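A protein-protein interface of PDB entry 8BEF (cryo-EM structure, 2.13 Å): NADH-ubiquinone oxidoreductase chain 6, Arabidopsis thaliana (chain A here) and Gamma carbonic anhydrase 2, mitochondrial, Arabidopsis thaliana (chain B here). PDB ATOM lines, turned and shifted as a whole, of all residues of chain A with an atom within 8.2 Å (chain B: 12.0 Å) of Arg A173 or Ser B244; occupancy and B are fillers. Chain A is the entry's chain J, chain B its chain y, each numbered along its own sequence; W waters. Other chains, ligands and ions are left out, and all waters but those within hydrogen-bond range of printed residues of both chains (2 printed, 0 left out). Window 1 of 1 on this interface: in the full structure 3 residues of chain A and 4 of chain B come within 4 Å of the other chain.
Hydrophobic or aromatic side chains of chain B that line the printed part of chain A: Met B245.
Among the printed residues, 6 pairs touch across the chains.
Among the printed residues, no Asp or Glu carboxylate lies within 4 Å of a Lys or Arg side-chain nitrogen of the other chain.
Among the printed residues, merely in contact across the chains: Met A171 with Met B245 (3.5 Å), His A172 with Ser B244 (3.4 Å), Arg A173 with Met B245 (3.3 Å), Arg A173 with Leu B246 (3.7 Å) and Arg A173 with Gly B247 (3.2 Å).
Arg A173 touches just these residues of chain B: Ser B244 (3.3 Å), Met B245 (3.3 Å), Leu B246 (3.7 Å) and Gly B247 (3.2 Å).
Of chain A, only His A172 and Arg A173 come within 4 Å of Ser B244.
Printed residues of chain A within 4 Å of Gly B247: Arg A173 (3.2 Å).
Of the printed residues of chain A, Met B245 touches Met A171 (3.5 Å) and Arg A173 (3.3 Å).
Printed residues of chain A within 4 Å of Leu B246: Arg A173.
Asp B243 touches none of the printed residues of chain A.
The nearest residue of chain B that does not touch Arg A173 is Ile B248 (5.4 Å).
The nearest printed residue of chain A that does not touch Leu B246 is Met A171 (5.8 Å).
O of Ser B244 is in hydrogen-bond range of N of Arg A173 (3.3 Å).
Water W1 bridges O of Arg A173 and O of Ser B244.
Water W2 bridges the backbone carbonyl oxygen (O) of Leu B246 (3.3 Å) and the guanidinium group (NH1) of Arg A173 (3.3 Å).
OG of Ser B244 is in hydrogen-bond range of O of Asp B241 (2.8 Å).
A ring nitrogen (ND1) of His A172 lies within hydrogen-bond range of the backbone carbonyl oxygen of Thr A170 (3.1 Å).
The backbone NH (N) of Arg A173 is in hydrogen-bond range of the side-chain sulfur (SD) of Met A171, at 3.6 Å.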
ATOM      1  N   ILE A 167      16.251  15.031 -22.831  1.00  0.00           N
ATOM      2  CA  ILE A 167      17.146  16.148 -22.528  1.00  0.00           C
ATOM      3  C   ILE A 167      18.064  16.447 -23.712  1.00  0.00           C
ATOM      4  O   ILE A 167      18.139  17.586 -24.182  1.00  0.00           O
ATOM      5  CB  ILE A 167      17.951  15.878 -21.246  1.00  0.00           C
ATOM      6  CG1 ILE A 167      17.035  15.879 -20.019  1.00  0.00           C
ATOM      7  CG2 ILE A 167      19.054  16.919 -21.100  1.00  0.00           C
ATOM      8  CD1 ILE A 167      16.056  17.028 -19.975  1.00  0.00           C
ATOM      9  N   THR A 170      16.282  18.110 -26.996  1.00  0.00           N
ATOM     10  CA  THR A 170      15.485  19.330 -26.971  1.00  0.00           C
ATOM     11  C   THR A 170      16.014  20.441 -26.071  1.00  0.00           C
ATOM     12  O   THR A 170      15.596  21.588 -26.249  1.00  0.00           O
ATOM     13  CB  THR A 170      14.037  19.023 -26.549  1.00  0.00           C
ATOM     14  OG1 THR A 170      14.020  18.515 -25.212  1.00  0.00           O
ATOM     15  CG2 THR A 170      13.410  17.998 -27.489  1.00  0.00           C
ATOM     16  N   MET A 171      16.911  20.151 -25.131  1.00  0.00           N
ATOM     17  CA  MET A 171      17.304  21.144 -24.136  1.00  0.00           C
ATOM     18  C   MET A 171      18.055  22.313 -24.767  1.00  0.00           C
ATOM     19  O   MET A 171      19.024  22.123 -25.507  1.00  0.00           O
ATOM     20  CB  MET A 171      18.170  20.495 -23.057  1.00  0.00           C
ATOM     21  CG  MET A 171      18.597  21.426 -21.929  1.00  0.00           C
ATOM     22  SD  MET A 171      17.363  22.668 -21.499  1.00  0.00           S
ATOM     23  CE  MET A 171      16.790  22.022 -19.933  1.00  0.00           C
ATOM     24  N   HIS A 172      17.600  23.526 -24.456  1.00  0.00           N
ATOM     25  CA  HIS A 172      18.311  24.771 -24.752  1.00  0.00           C
ATOM     26  C   HIS A 172      18.294  25.568 -23.450  1.00  0.00           C
ATOM     27  O   HIS A 172      17.314  26.255 -23.154  1.00  0.00           O
ATOM     28  CB  HIS A 172      17.662  25.543 -25.899  1.00  0.00           C
ATOM     29  CG  HIS A 172      17.909  24.950 -27.250  1.00  0.00           C
ATOM     30  ND1 HIS A 172      17.250  23.828 -27.703  1.00  0.00           N
ATOM     31  CD2 HIS A 172      18.741  25.325 -28.249  1.00  0.00           C
ATOM     32  CE1 HIS A 172      17.668  23.537 -28.921  1.00  0.00           C
ATOM     33  NE2 HIS A 172      18.574  24.429 -29.275  1.00  0.00           N
ATOM     34  N   ARG A 173      19.365  25.460 -22.668  1.00  0.00           N
ATOM     35  CA  ARG A 173      19.403  26.099 -21.360  1.00  0.00           C
ATOM     36  C   ARG A 173      19.561  27.608 -21.514  1.00  0.00           C
ATOM     37  O   ARG A 173      20.412  28.081 -22.273  1.00  0.00           O
ATOM     38  CB  ARG A 173      20.544  25.524 -20.520  1.00  0.00           C
ATOM     39  CG  ARG A 173      20.452  25.839 -19.033  1.00  0.00           C
ATOM     40  CD  ARG A 173      21.513  25.092 -18.238  1.00  0.00           C
ATOM     41  NE  ARG A 173      21.214  25.065 -16.812  1.00  0.00           N
ATOM     42  CZ  ARG A 173      21.707  24.177 -15.960  1.00  0.00           C
ATOM     43  NH1 ARG A 173      22.531  23.221 -16.356  1.00  0.00           N
ATOM     44  NH2 ARG A 173      21.361  24.247 -14.677  1.00  0.00           N
ATOM     45  N   THR A 174      18.740  28.361 -20.794  1.00  0.00           N
ATOM     46  CA  THR A 174      18.785  29.816 -20.875  1.00  0.00           C
ATOM     47  C   THR A 174      20.066  30.361 -20.252  1.00  0.00           C
ATOM     48  O   THR A 174      20.893  30.960 -20.943  1.00  0.00           O
ATOM     49  CB  THR A 174      17.572  30.459 -20.183  1.00  0.00           C
ATOM     50  OG1 THR A 174      16.365  29.913 -20.729  1.00  0.00           O
ATOM     51  CG2 THR A 174      17.580  31.964 -20.394  1.00  0.00           C
ATOM     52  N   LYS B 238      34.515  24.011 -33.039  1.00  0.00           N
ATOM     53  CA  LYS B 238      33.428  24.399 -32.150  1.00  0.00           C
ATOM     54  C   LYS B 238      32.307  23.370 -32.199  1.00  0.00           C
ATOM     55  O   LYS B 238      32.173  22.609 -33.160  1.00  0.00           O
ATOM     56  CB  LYS B 238      32.879  25.787 -32.508  1.00  0.00           C
ATOM     57  CG  LYS B 238      32.945  26.120 -33.987  1.00  0.00           C
ATOM     58  CD  LYS B 238      32.505  27.553 -34.255  1.00  0.00           C
ATOM     59  CE  LYS B 238      33.522  28.557 -33.739  1.00  0.00           C
ATOM     60  NZ  LYS B 238      33.217  29.938 -34.207  1.00  0.00           N
ATOM     61  N   ASP B 239      31.509  23.342 -31.112  1.00  0.00           N
ATOM     62  CA  ASP B 239      30.206  22.665 -31.077  1.00  0.00           C
ATOM     63  C   ASP B 239      29.219  23.644 -30.445  1.00  0.00           C
ATOM     64  O   ASP B 239      28.911  23.562 -29.255  1.00  0.00           O
ATOM     65  CB  ASP B 239      30.263  21.357 -30.296  1.00  0.00           C
ATOM     66  CG  ASP B 239      28.980  20.540 -30.403  1.00  0.00           C
ATOM     67  OD1 ASP B 239      28.019  20.989 -31.064  1.00  0.00           O
ATOM     68  OD2 ASP B 239      28.939  19.432 -29.831  1.00  0.00           O
ATOM     69  N   GLU B 240      28.690  24.554 -31.263  1.00  0.00           N
ATOM     70  CA  GLU B 240      27.786  25.569 -30.742  1.00  0.00           C
ATOM     71  C   GLU B 240      26.447  24.985 -30.315  1.00  0.00           C
ATOM     72  O   GLU B 240      25.790  25.549 -29.437  1.00  0.00           O
ATOM     73  CB  GLU B 240      27.576  26.666 -31.783  1.00  0.00           C
ATOM     74  CG  GLU B 240      28.857  27.356 -32.209  1.00  0.00           C
ATOM     75  CD  GLU B 240      28.628  28.790 -32.645  1.00  0.00           C
ATOM     76  OE1 GLU B 240      29.060  29.148 -33.761  1.00  0.00           O
ATOM     77  OE2 GLU B 240      28.017  29.557 -31.872  1.00  0.00           O
ATOM     78  N   ASP B 241      26.036  23.867 -30.910  1.00  0.00           N
ATOM     79  CA  ASP B 241      24.791  23.229 -30.503  1.00  0.00           C
ATOM     80  C   ASP B 241      24.877  22.690 -29.078  1.00  0.00           C
ATOM     81  O   ASP B 241      23.955  22.884 -28.275  1.00  0.00           O
ATOM     82  CB  ASP B 241      24.446  22.114 -31.484  1.00  0.00           C
ATOM     83  CG  ASP B 241      23.060  21.574 -31.276  1.00  0.00           C
ATOM     84  OD1 ASP B 241      22.166  22.354 -30.890  1.00  0.00           O
ATOM     85  OD2 ASP B 241      22.872  20.364 -31.489  1.00  0.00           O
ATOM     86  N   TYR B 242      25.983  22.027 -28.737  1.00  0.00           N
ATOM     87  CA  TYR B 242      26.145  21.551 -27.368  1.00  0.00           C
ATOM     88  C   TYR B 242      26.327  22.704 -26.394  1.00  0.00           C
ATOM     89  O   TYR B 242      25.897  22.607 -25.241  1.00  0.00           O
ATOM     90  CB  TYR B 242      27.322  20.586 -27.261  1.00  0.00           C
ATOM     91  CG  TYR B 242      27.231  19.670 -26.061  1.00  0.00           C
ATOM     92  CD1 TYR B 242      26.332  18.612 -26.042  1.00  0.00           C
ATOM     93  CD2 TYR B 242      28.033  19.872 -24.946  1.00  0.00           C
ATOM     94  CE1 TYR B 242      26.242  17.774 -24.954  1.00  0.00           C
ATOM     95  CE2 TYR B 242      27.951  19.035 -23.845  1.00  0.00           C
ATOM     96  CZ  TYR B 242      27.052  17.987 -23.855  1.00  0.00           C
ATOM     97  OH  TYR B 242      26.959  17.149 -22.771  1.00  0.00           O
ATOM     98  N   ASP B 243      26.968  23.792 -26.829  1.00  0.00           N
ATOM     99  CA  ASP B 243      27.053  24.978 -25.983  1.00  0.00           C
ATOM    100  C   ASP B 243      25.670  25.549 -25.699  1.00  0.00           C
ATOM    101  O   ASP B 243      25.373  25.938 -24.565  1.00  0.00           O
ATOM    102  CB  ASP B 243      27.944  26.035 -26.635  1.00  0.00           C
ATOM    103  CG  ASP B 243      29.415  25.675 -26.575  1.00  0.00           C
ATOM    104  OD1 ASP B 243      30.016  25.428 -27.639  1.00  0.00           O
ATOM    105  OD2 ASP B 243      29.970  25.630 -25.460  1.00  0.00           O
ATOM    106  N   SER B 244      24.811  25.604 -26.719  1.00  0.00           N
ATOM    107  CA  SER B 244      23.446  26.075 -26.507  1.00  0.00           C
ATOM    108  C   SER B 244      22.693  25.150 -25.560  1.00  0.00           C
ATOM    109  O   SER B 244      21.898  25.611 -24.734  1.00  0.00           O
ATOM    110  CB  SER B 244      22.714  26.203 -27.843  1.00  0.00           C
ATOM    111  OG  SER B 244      22.089  24.987 -28.206  1.00  0.00           O
ATOM    112  N   MET B 245      22.930  23.838 -25.662  1.00  0.00           N
ATOM    113  CA  MET B 245      22.355  22.927 -24.676  1.00  0.00           C
ATOM    114  C   MET B 245      22.860  23.250 -23.274  1.00  0.00           C
ATOM    115  O   MET B 245      22.085  23.253 -22.312  1.00  0.00           O
ATOM    116  CB  MET B 245      22.664  21.470 -25.028  1.00  0.00           C
ATOM    117  CG  MET B 245      21.854  20.474 -24.198  1.00  0.00           C
ATOM    118  SD  MET B 245      22.575  18.825 -24.059  1.00  0.00           S
ATOM    119  CE  MET B 245      23.911  19.133 -22.914  1.00  0.00           C
ATOM    120  N   LEU B 246      24.158  23.531 -23.143  1.00  0.00           N
ATOM    121  CA  LEU B 246      24.725  23.912 -21.855  1.00  0.00           C
ATOM    122  C   LEU B 246      24.351  25.333 -21.457  1.00  0.00           C
ATOM    123  O   LEU B 246      24.521  25.699 -20.291  1.00  0.00           O
ATOM    124  CB  LEU B 246      26.250  23.773 -21.886  1.00  0.00           C
ATOM    125  CG  LEU B 246      26.847  22.368 -21.766  1.00  0.00           C
ATOM    126  CD1 LEU B 246      28.288  22.341 -22.264  1.00  0.00           C
ATOM    127  CD2 LEU B 246      26.770  21.880 -20.332  1.00  0.00           C
ATOM    128  N   GLY B 247      23.847  26.133 -22.390  1.00  0.00           N
ATOM    129  CA  GLY B 247      23.541  27.525 -22.110  1.00  0.00           C
ATOM    130  C   GLY B 247      24.754  28.396 -21.863  1.00  0.00           C
ATOM    131  O   GLY B 247      24.722  29.262 -20.982  1.00  0.00           O
ATOM    132  N   ILE B 248      25.830  28.186 -22.621  1.00  0.00           N
ATOM    133  CA  ILE B 248      27.042  28.984 -22.506  1.00  0.00           C
ATOM    134  C   ILE B 248      27.448  29.449 -23.895  1.00  0.00           C
ATOM    135  O   ILE B 248      27.029  28.892 -24.912  1.00  0.00           O
ATOM    136  CB  ILE B 248      28.207  28.211 -21.849  1.00  0.00           C
ATOM    137  CG1 ILE B 248      28.672  27.077 -22.766  1.00  0.00           C
ATOM    138  CG2 ILE B 248      27.808  27.689 -20.480  1.00  0.00           C
ATOM    139  CD1 ILE B 248      30.062  26.574 -22.463  1.00  0.00           C
ATOM    140  N   THR B 249      28.288  30.478 -23.928  1.00  0.00           N
ATOM    141  CA  THR B 249      28.793  31.028 -25.181  1.00  0.00           C
ATOM    142  C   THR B 249      30.300  31.183 -25.062  1.00  0.00           C
ATOM    143  O   THR B 249      30.785  32.035 -24.310  1.00  0.00           O
ATOM    144  CB  THR B 249      28.129  32.360 -25.513  1.00  0.00           C
ATOM    145  OG1 THR B 249      26.734  32.147 -25.755  1.00  0.00           O
ATOM    146  CG2 THR B 249      28.762  32.965 -26.753  1.00  0.00           C
ATOM    147  N   ARG B 250      31.034  30.359 -25.799  1.00  0.00           N
ATOM    148  CA  ARG B 250      32.486  30.412 -25.785  1.00  0.00           C
ATOM    149  C   ARG B 250      32.959  31.590 -26.622  1.00  0.00           C
ATOM    150  O   ARG B 250      32.540  31.755 -27.771  1.00  0.00           O
ATOM    151  CB  ARG B 250      33.065  29.101 -26.315  1.00  0.00           C
ATOM    152  CG  ARG B 250      32.447  27.875 -25.663  1.00  0.00           C
ATOM    153  CD  ARG B 250      33.324  26.656 -25.809  1.00  0.00           C
ATOM    154  NE  ARG B 250      32.670  25.457 -25.297  1.00  0.00           N
ATOM    155  CZ  ARG B 250      32.852  24.973 -24.077  1.00  0.00           C
ATOM    156  NH1 ARG B 250      33.646  25.573 -23.207  1.00  0.00           N
ATOM    157  NH2 ARG B 250      32.222  23.856 -23.722  1.00  0.00           N
ATOM    158  N   GLU B 251      33.824  32.412 -26.042  1.00  0.00           N
ATOM    159  CA  GLU B 251      34.347  33.593 -26.707  1.00  0.00           C
ATOM    160  C   GLU B 251      35.821  33.395 -27.026  1.00  0.00           C
ATOM    161  O   GLU B 251      36.560  32.797 -26.239  1.00  0.00           O
ATOM    162  CB  GLU B 251      34.155  34.841 -25.840  1.00  0.00           C
ATOM    163  CG  GLU B 251      32.713  35.399 -25.717  1.00  0.00           C
ATOM    164  CD  GLU B 251      31.954  35.626 -27.034  1.00  0.00           C
ATOM    165  OE1 GLU B 251      32.232  34.986 -28.069  1.00  0.00           O
ATOM    166  OE2 GLU B 251      31.038  36.476 -27.023  1.00  0.00           O
HETATM  167  O   HOH W   1      20.678  28.006 -24.768  1.00  0.00           O
HETATM  168  O   HOH W   2      25.502  23.792 -17.788  1.00  0.00           O
